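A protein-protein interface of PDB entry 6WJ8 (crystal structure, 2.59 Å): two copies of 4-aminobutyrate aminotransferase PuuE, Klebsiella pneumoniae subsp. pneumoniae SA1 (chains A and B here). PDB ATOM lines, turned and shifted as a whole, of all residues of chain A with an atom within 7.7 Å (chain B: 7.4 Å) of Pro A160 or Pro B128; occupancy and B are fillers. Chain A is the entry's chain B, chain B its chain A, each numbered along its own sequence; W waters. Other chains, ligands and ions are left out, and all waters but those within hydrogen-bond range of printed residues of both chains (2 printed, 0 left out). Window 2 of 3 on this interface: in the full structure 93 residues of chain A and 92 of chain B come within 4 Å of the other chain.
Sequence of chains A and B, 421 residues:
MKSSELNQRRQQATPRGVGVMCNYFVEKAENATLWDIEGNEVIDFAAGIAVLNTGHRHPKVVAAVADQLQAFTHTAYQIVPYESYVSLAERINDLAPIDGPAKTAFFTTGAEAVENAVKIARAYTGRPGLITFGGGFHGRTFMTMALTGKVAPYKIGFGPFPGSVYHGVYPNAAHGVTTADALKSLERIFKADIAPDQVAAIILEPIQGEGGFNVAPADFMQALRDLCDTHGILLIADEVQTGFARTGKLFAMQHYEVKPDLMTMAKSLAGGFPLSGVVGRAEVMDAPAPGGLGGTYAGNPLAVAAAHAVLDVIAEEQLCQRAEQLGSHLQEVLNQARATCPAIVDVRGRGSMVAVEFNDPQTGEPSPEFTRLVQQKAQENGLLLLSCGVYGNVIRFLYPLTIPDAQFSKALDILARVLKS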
ATOM      1  N   PHE A 142      32.677  27.539  32.672  1.00  0.00           N
ATOM      2  CA  PHE A 142      31.650  27.322  31.654  1.00  0.00           C
ATOM      3  C   PHE A 142      31.140  28.637  31.079  1.00  0.00           C
ATOM      4  O   PHE A 142      31.142  28.839  29.859  1.00  0.00           O
ATOM      5  CB  PHE A 142      30.496  26.511  32.241  1.00  0.00           C
ATOM      6  CG  PHE A 142      29.459  26.111  31.232  1.00  0.00           C
ATOM      7  CD1 PHE A 142      28.121  26.396  31.444  1.00  0.00           C
ATOM      8  CD2 PHE A 142      29.823  25.449  30.071  1.00  0.00           C
ATOM      9  CE1 PHE A 142      27.164  26.028  30.518  1.00  0.00           C
ATOM     10  CE2 PHE A 142      28.871  25.079  29.141  1.00  0.00           C
ATOM     11  CZ  PHE A 142      27.540  25.366  29.365  1.00  0.00           C
ATOM     12  N   ALA A 146      32.182  30.580  27.472  1.00  0.00           N
ATOM     13  CA  ALA A 146      31.209  31.098  26.518  1.00  0.00           C
ATOM     14  C   ALA A 146      31.449  32.576  26.241  1.00  0.00           C
ATOM     15  O   ALA A 146      31.278  33.037  25.106  1.00  0.00           O
ATOM     16  CB  ALA A 146      29.790  30.872  27.041  1.00  0.00           C
ATOM     17  N   LYS A 155      37.846  26.459  24.339  1.00  0.00           N
ATOM     18  CA  LYS A 155      36.488  25.933  24.333  1.00  0.00           C
ATOM     19  C   LYS A 155      36.339  24.616  23.585  1.00  0.00           C
ATOM     20  O   LYS A 155      35.224  24.085  23.521  1.00  0.00           O
ATOM     21  CB  LYS A 155      35.529  26.972  23.737  1.00  0.00           C
ATOM     22  CG  LYS A 155      35.690  28.360  24.340  1.00  0.00           C
ATOM     23  CD  LYS A 155      35.142  29.442  23.426  1.00  0.00           C
ATOM     24  CE  LYS A 155      33.632  29.353  23.310  1.00  0.00           C
ATOM     25  NZ  LYS A 155      33.017  30.701  23.150  1.00  0.00           N
ATOM     26  N   GLY A 157      35.922  20.992  23.016  1.00  0.00           N
ATOM     27  CA  GLY A 157      35.602  19.788  23.753  1.00  0.00           C
ATOM     28  C   GLY A 157      34.828  19.983  25.038  1.00  0.00           C
ATOM     29  O   GLY A 157      34.607  19.003  25.760  1.00  0.00           O
ATOM     30  N   PHE A 158      34.404  21.207  25.351  1.00  0.00           N
ATOM     31  CA  PHE A 158      33.678  21.479  26.586  1.00  0.00           C
ATOM     32  C   PHE A 158      32.264  21.987  26.337  1.00  0.00           C
ATOM     33  O   PHE A 158      31.592  22.406  27.289  1.00  0.00           O
ATOM     34  CB  PHE A 158      34.455  22.478  27.448  1.00  0.00           C
ATOM     35  CG  PHE A 158      35.927  22.190  27.528  1.00  0.00           C
ATOM     36  CD1 PHE A 158      36.382  20.975  28.015  1.00  0.00           C
ATOM     37  CD2 PHE A 158      36.854  23.130  27.113  1.00  0.00           C
ATOM     38  CE1 PHE A 158      37.736  20.705  28.088  1.00  0.00           C
ATOM     39  CE2 PHE A 158      38.209  22.866  27.183  1.00  0.00           C
ATOM     40  CZ  PHE A 158      38.651  21.652  27.672  1.00  0.00           C
ATOM     41  N   GLY A 159      31.791  21.962  25.089  1.00  0.00           N
ATOM     42  CA  GLY A 159      30.445  22.361  24.795  1.00  0.00           C
ATOM     43  C   GLY A 159      29.437  21.312  25.229  1.00  0.00           C
ATOM     44  O   GLY A 159      29.792  20.266  25.788  1.00  0.00           O
ATOM     45  N   PRO A 160      28.148  21.588  24.976  1.00  0.00           N
ATOM     46  CA  PRO A 160      27.620  22.810  24.362  1.00  0.00           C
ATOM     47  C   PRO A 160      27.512  23.956  25.361  1.00  0.00           C
ATOM     48  O   PRO A 160      27.438  23.722  26.566  1.00  0.00           O
ATOM     49  CB  PRO A 160      26.239  22.378  23.873  1.00  0.00           C
ATOM     50  CG  PRO A 160      25.821  21.350  24.859  1.00  0.00           C
ATOM     51  CD  PRO A 160      27.078  20.620  25.266  1.00  0.00           C
ATOM     52  N   PHE A 161      27.494  25.175  24.856  1.00  0.00           N
ATOM     53  CA  PHE A 161      27.564  26.373  25.673  1.00  0.00           C
ATOM     54  C   PHE A 161      26.199  27.039  25.778  1.00  0.00           C
ATOM     55  O   PHE A 161      25.318  26.811  24.942  1.00  0.00           O
ATOM     56  CB  PHE A 161      28.599  27.336  25.081  1.00  0.00           C
ATOM     57  CG  PHE A 161      30.013  26.856  25.237  1.00  0.00           C
ATOM     58  CD1 PHE A 161      30.688  27.027  26.434  1.00  0.00           C
ATOM     59  CD2 PHE A 161      30.660  26.211  24.194  1.00  0.00           C
ATOM     60  CE1 PHE A 161      31.986  26.578  26.586  1.00  0.00           C
ATOM     61  CE2 PHE A 161      31.958  25.759  24.339  1.00  0.00           C
ATOM     62  CZ  PHE A 161      32.622  25.943  25.537  1.00  0.00           C
ATOM     63  N   PRO A 162      25.977  27.862  26.803  1.00  0.00           N
ATOM     64  CA  PRO A 162      24.626  28.377  27.052  1.00  0.00           C
ATOM     65  C   PRO A 162      24.189  29.385  26.000  1.00  0.00           C
ATOM     66  O   PRO A 162      24.996  29.968  25.273  1.00  0.00           O
ATOM     67  CB  PRO A 162      24.749  29.038  28.428  1.00  0.00           C
ATOM     68  CG  PRO A 162      26.175  29.449  28.505  1.00  0.00           C
ATOM     69  CD  PRO A 162      26.938  28.362  27.805  1.00  0.00           C
ATOM     70  N   GLY A 163      22.874  29.579  25.932  1.00  0.00           N
ATOM     71  CA  GLY A 163      22.296  30.576  25.061  1.00  0.00           C
ATOM     72  C   GLY A 163      22.419  31.971  25.636  1.00  0.00           C
ATOM     73  O   GLY A 163      23.006  32.197  26.694  1.00  0.00           O
ATOM     74  N   ALA B 121      35.034  15.518  32.016  1.00  0.00           N
ATOM     75  CA  ALA B 121      34.005  14.530  31.706  1.00  0.00           C
ATOM     76  C   ALA B 121      33.359  14.810  30.354  1.00  0.00           C
ATOM     77  O   ALA B 121      33.075  13.880  29.590  1.00  0.00           O
ATOM     78  CB  ALA B 121      32.952  14.505  32.812  1.00  0.00           C
ATOM     79  N   ARG B 122      33.119  16.087  30.041  1.00  0.00           N
ATOM     80  CA  ARG B 122      32.539  16.425  28.745  1.00  0.00           C
ATOM     81  C   ARG B 122      33.516  16.139  27.613  1.00  0.00           C
ATOM     82  O   ARG B 122      33.115  15.659  26.546  1.00  0.00           O
ATOM     83  CB  ARG B 122      32.108  17.892  28.727  1.00  0.00           C
ATOM     84  CG  ARG B 122      30.770  18.150  29.403  1.00  0.00           C
ATOM     85  CD  ARG B 122      30.283  19.566  29.151  1.00  0.00           C
ATOM     86  NE  ARG B 122      28.848  19.693  29.385  1.00  0.00           N
ATOM     87  CZ  ARG B 122      28.150  20.805  29.174  1.00  0.00           C
ATOM     88  NH1 ARG B 122      28.756  21.893  28.723  1.00  0.00           N
ATOM     89  NH2 ARG B 122      26.847  20.827  29.415  1.00  0.00           N
ATOM     90  N   THR B 125      33.642  12.010  27.377  1.00  0.00           N
ATOM     91  CA  THR B 125      32.444  11.338  26.892  1.00  0.00           C
ATOM     92  C   THR B 125      31.851  11.988  25.652  1.00  0.00           C
ATOM     93  O   THR B 125      31.134  11.317  24.901  1.00  0.00           O
ATOM     94  CB  THR B 125      31.378  11.302  27.991  1.00  0.00           C
ATOM     95  OG1 THR B 125      30.998  12.640  28.331  1.00  0.00           O
ATOM     96  CG2 THR B 125      31.914  10.605  29.233  1.00  0.00           C
ATOM     97  N   GLY B 126      32.132  13.269  25.414  1.00  0.00           N
ATOM     98  CA  GLY B 126      31.481  13.979  24.334  1.00  0.00           C
ATOM     99  C   GLY B 126      30.006  14.225  24.545  1.00  0.00           C
ATOM    100  O   GLY B 126      29.308  14.577  23.589  1.00  0.00           O
ATOM    101  N   ARG B 127      29.509  14.051  25.772  1.00  0.00           N
ATOM    102  CA  ARG B 127      28.106  14.179  26.121  1.00  0.00           C
ATOM    103  C   ARG B 127      27.852  15.470  26.896  1.00  0.00           C
ATOM    104  O   ARG B 127      28.748  15.984  27.572  1.00  0.00           O
ATOM    105  CB  ARG B 127      27.642  12.987  26.965  1.00  0.00           C
ATOM    106  CG  ARG B 127      28.003  11.632  26.382  1.00  0.00           C
ATOM    107  CD  ARG B 127      27.804  10.534  27.411  1.00  0.00           C
ATOM    108  NE  ARG B 127      27.983   9.203  26.841  1.00  0.00           N
ATOM    109  CZ  ARG B 127      27.638   8.078  27.456  1.00  0.00           C
ATOM    110  NH1 ARG B 127      27.093   8.123  28.664  1.00  0.00           N
ATOM    111  NH2 ARG B 127      27.837   6.908  26.866  1.00  0.00           N
ATOM    112  N   PRO B 128      26.639  16.018  26.814  1.00  0.00           N
ATOM    113  CA  PRO B 128      26.345  17.274  27.517  1.00  0.00           C
ATOM    114  C   PRO B 128      25.741  17.079  28.900  1.00  0.00           C
ATOM    115  O   PRO B 128      25.747  18.004  29.719  1.00  0.00           O
ATOM    116  CB  PRO B 128      25.345  17.955  26.579  1.00  0.00           C
ATOM    117  CG  PRO B 128      24.599  16.814  25.964  1.00  0.00           C
ATOM    118  CD  PRO B 128      25.565  15.651  25.872  1.00  0.00           C
ATOM    119  N   GLY B 129      25.219  15.886  29.170  1.00  0.00           N
ATOM    120  CA  GLY B 129      24.378  15.700  30.341  1.00  0.00           C
ATOM    121  C   GLY B 129      25.170  15.700  31.638  1.00  0.00           C
ATOM    122  O   GLY B 129      26.280  15.174  31.721  1.00  0.00           O
ATOM    123  N   LEU B 130      24.575  16.304  32.665  1.00  0.00           N
ATOM    124  CA  LEU B 130      25.121  16.307  34.016  1.00  0.00           C
ATOM    125  C   LEU B 130      23.969  16.154  34.997  1.00  0.00           C
ATOM    126  O   LEU B 130      22.990  16.900  34.923  1.00  0.00           O
ATOM    127  CB  LEU B 130      25.897  17.596  34.306  1.00  0.00           C
ATOM    128  CG  LEU B 130      27.123  17.891  33.439  1.00  0.00           C
ATOM    129  CD1 LEU B 130      27.539  19.348  33.576  1.00  0.00           C
ATOM    130  CD2 LEU B 130      28.272  16.964  33.801  1.00  0.00           C
ATOM    131  N   ILE B 131      24.083  15.190  35.907  1.00  0.00           N
ATOM    132  CA  ILE B 131      23.048  14.916  36.897  1.00  0.00           C
ATOM    133  C   ILE B 131      23.646  15.080  38.286  1.00  0.00           C
ATOM    134  O   ILE B 131      24.663  14.453  38.608  1.00  0.00           O
ATOM    135  CB  ILE B 131      22.449  13.507  36.729  1.00  0.00           C
ATOM    136  CG1 ILE B 131      21.865  13.332  35.326  1.00  0.00           C
ATOM    137  CG2 ILE B 131      21.381  13.257  37.782  1.00  0.00           C
ATOM    138  CD1 ILE B 131      21.259  11.964  35.088  1.00  0.00           C
ATOM    139  N   MET B 143      27.894  27.368  36.069  1.00  0.00           N
ATOM    140  CA  MET B 143      27.675  25.931  35.935  1.00  0.00           C
ATOM    141  C   MET B 143      27.513  25.264  37.295  1.00  0.00           C
ATOM    142  O   MET B 143      26.645  24.401  37.468  1.00  0.00           O
ATOM    143  CB  MET B 143      28.827  25.295  35.159  1.00  0.00           C
ATOM    144  CG  MET B 143      28.853  23.776  35.209  1.00  0.00           C
ATOM    145  SD  MET B 143      27.377  23.020  34.498  1.00  0.00           S
ATOM    146  CE  MET B 143      27.745  23.130  32.749  1.00  0.00           C
ATOM    147  N   PRO B 162      21.875  26.608  32.329  1.00  0.00           N
ATOM    148  CA  PRO B 162      22.089  25.823  31.110  1.00  0.00           C
ATOM    149  C   PRO B 162      21.306  24.524  31.134  1.00  0.00           C
ATOM    150  O   PRO B 162      21.041  23.946  32.192  1.00  0.00           O
ATOM    151  CB  PRO B 162      23.598  25.564  31.120  1.00  0.00           C
ATOM    152  CG  PRO B 162      23.940  25.524  32.563  1.00  0.00           C
ATOM    153  CD  PRO B 162      23.037  26.529  33.234  1.00  0.00           C
ATOM    154  N   GLY B 163      20.930  24.070  29.946  1.00  0.00           N
ATOM    155  CA  GLY B 163      20.222  22.819  29.805  1.00  0.00           C
ATOM    156  C   GLY B 163      21.107  21.626  30.116  1.00  0.00           C
ATOM    157  O   GLY B 163      22.286  21.744  30.453  1.00  0.00           O
ATOM    158  N   SER B 164      20.499  20.443  30.008  1.00  0.00           N
ATOM    159  CA  SER B 164      21.187  19.166  30.206  1.00  0.00           C
ATOM    160  C   SER B 164      21.742  19.025  31.622  1.00  0.00           C
ATOM    161  O   SER B 164      22.708  18.292  31.850  1.00  0.00           O
ATOM    162  CB  SER B 164      22.305  18.971  29.175  1.00  0.00           C
ATOM    163  OG  SER B 164      21.785  18.919  27.859  1.00  0.00           O
ATOM    164  N   VAL B 165      21.143  19.720  32.587  1.00  0.00           N
ATOM    165  CA  VAL B 165      21.536  19.630  33.990  1.00  0.00           C
ATOM    166  C   VAL B 165      20.272  19.396  34.806  1.00  0.00           C
ATOM    167  O   VAL B 165      19.400  20.272  34.871  1.00  0.00           O
ATOM    168  CB  VAL B 165      22.275  20.882  34.478  1.00  0.00           C
ATOM    169  CG1 VAL B 165      22.555  20.779  35.970  1.00  0.00           C
ATOM    170  CG2 VAL B 165      23.572  21.072  33.703  1.00  0.00           C
ATOM    171  N   ILE B 194      16.663  13.303  29.966  1.00  0.00           N
ATOM    172  CA  ILE B 194      17.789  13.122  29.059  1.00  0.00           C
ATOM    173  C   ILE B 194      18.141  11.642  29.005  1.00  0.00           C
ATOM    174  O   ILE B 194      18.050  10.930  30.011  1.00  0.00           O
ATOM    175  CB  ILE B 194      18.992  13.985  29.501  1.00  0.00           C
ATOM    176  CG1 ILE B 194      20.176  13.812  28.548  1.00  0.00           C
ATOM    177  CG2 ILE B 194      19.383  13.668  30.940  1.00  0.00           C
ATOM    178  CD1 ILE B 194      21.228  14.884  28.689  1.00  0.00           C
ATOM    179  N   ASP B 197      22.758   7.655  27.635  1.00  0.00           N
ATOM    180  CA  ASP B 197      23.968   7.791  26.834  1.00  0.00           C
ATOM    181  C   ASP B 197      24.265   9.235  26.444  1.00  0.00           C
ATOM    182  O   ASP B 197      25.240   9.475  25.725  1.00  0.00           O
ATOM    183  CB  ASP B 197      23.874   6.917  25.581  1.00  0.00           C
ATOM    184  CG  ASP B 197      22.832   7.411  24.609  1.00  0.00           C
ATOM    185  OD1 ASP B 197      23.118   7.441  23.394  1.00  0.00           O
ATOM    186  OD2 ASP B 197      21.726   7.771  25.063  1.00  0.00           O
ATOM    187  N   GLN B 198      23.457  10.196  26.892  1.00  0.00           N
ATOM    188  CA  GLN B 198      23.748  11.611  26.716  1.00  0.00           C
ATOM    189  C   GLN B 198      24.155  12.290  28.015  1.00  0.00           C
ATOM    190  O   GLN B 198      24.391  13.503  28.017  1.00  0.00           O
ATOM    191  CB  GLN B 198      22.538  12.335  26.112  1.00  0.00           C
ATOM    192  CG  GLN B 198      22.215  11.918  24.687  1.00  0.00           C
ATOM    193  CD  GLN B 198      23.377  12.141  23.737  1.00  0.00           C
ATOM    194  OE1 GLN B 198      23.937  13.234  23.667  1.00  0.00           O
ATOM    195  NE2 GLN B 198      23.745  11.099  23.000  1.00  0.00           N
ATOM    196  N   VAL B 199      24.239  11.546  29.112  1.00  0.00           N
ATOM    197  CA  VAL B 199      24.683  12.082  30.393  1.00  0.00           C
ATOM    198  C   VAL B 199      26.184  11.856  30.507  1.00  0.00           C
ATOM    199  O   VAL B 199      26.654  10.714  30.463  1.00  0.00           O
ATOM    200  CB  VAL B 199      23.933  11.426  31.561  1.00  0.00           C
ATOM    201  CG1 VAL B 199      24.515  11.877  32.893  1.00  0.00           C
ATOM    202  CG2 VAL B 199      22.449  11.740  31.482  1.00  0.00           C
ATOM    203  N   ALA B 200      26.940  12.944  30.647  1.00  0.00           N
ATOM    204  CA  ALA B 200      28.392  12.826  30.720  1.00  0.00           C
ATOM    205  C   ALA B 200      28.848  12.348  32.092  1.00  0.00           C
ATOM    206  O   ALA B 200      29.803  11.571  32.193  1.00  0.00           O
ATOM    207  CB  ALA B 200      29.048  14.164  30.379  1.00  0.00           C
ATOM    208  N   ALA B 201      28.181  12.792  33.155  1.00  0.00           N
ATOM    209  CA  ALA B 201      28.634  12.463  34.498  1.00  0.00           C
ATOM    210  C   ALA B 201      27.485  12.595  35.486  1.00  0.00           C
ATOM    211  O   ALA B 201      26.582  13.416  35.307  1.00  0.00           O
ATOM    212  CB  ALA B 201      29.798  13.364  34.926  1.00  0.00           C
HETATM  213  O   HOH W   1      30.393  28.772  34.840  1.00  0.00           O
HETATM  214  O   HOH W   2      31.008  17.494  24.643  1.00  0.00           O
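The guanidinium group (NH1) of Arg B122 lies within hydrogen-bond range of the backbone carbonyl oxygen (O) of Phe A158 (3.2 Å). The guanidinium group (NH1) of Arg B122 lies within hydrogen-bond range of the backbone carbonyl oxygen (O) of Pro A160, at 3.1 Å.
The guanidinium group of Arg B122 sits at hydrogen-bond distance from the backbone carbonyl oxygen of Pro B128 (3.0 Å).
Among the printed residues, merely in contact across the chains: Phe A142 with Arg B122 (3.2 Å), Pro A160 with Pro B128 (3.4 Å), Gly A159 with Arg B122 (3.5 Å), Phe A142 with Met B143 (3.5 Å), Gly A157 with Arg B122 (3.6 Å) and Phe A142 with Pro B162 (3.6 Å).
Of chain B, only Arg B122 (3.1 Å) and Pro B128 (3.4 Å) come within 4 Å of Pro A160. Pro B128 touches just one residue of chain A: Pro A160 (3.4 Å). Of the printed residues of chain B, Gly A159 touches Arg B122 (3.5 Å). Of the printed residues of chain A, Arg B122 touches Phe A142, Gly A157, Phe A158, Gly A159 and Pro A160. Printed residues of chain A within 4 Å of Pro B162: Phe A142. The nearest residue of chain B that does not touch Pro A160 is Arg B127 (5.4 Å). The nearest residue of chain A that does not touch Pro B128 is Gly A159 (4.9 Å).
Of the 20 printed residues of chain B, 4 touch a printed residue of chain A. Of the 10 printed residues of chain A, 5 touch a printed residue of chain B. Printed residues of chain A that touch a printed residue of chain B: Phe A142, Gly A157, Phe A158, Gly A159 and Pro A160. Hydrophobic or aromatic side chains of chain A that line the printed part of chain B: Phe A142 and Pro A160. Among the printed residues, 8 pairs touch across the chains. Among the printed residues, no Asp or Glu carboxylate lies within 4 Å of a Lys or Arg side-chain nitrogen of the other chain.
Positions printed for both chains: 162 and 163. Of the 8 pairs that touch across the chains among the printed residues, none has its exchanged pair printed and touching as well.
Water W1 lies within hydrogen-bond range of N of Met B143 and N of Phe A142. Water W2 lies within hydrogen-bond range of the backbone carbonyl oxygen (O) of Gly A159 and the backbone carbonyl oxygen (O) of Arg B122.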
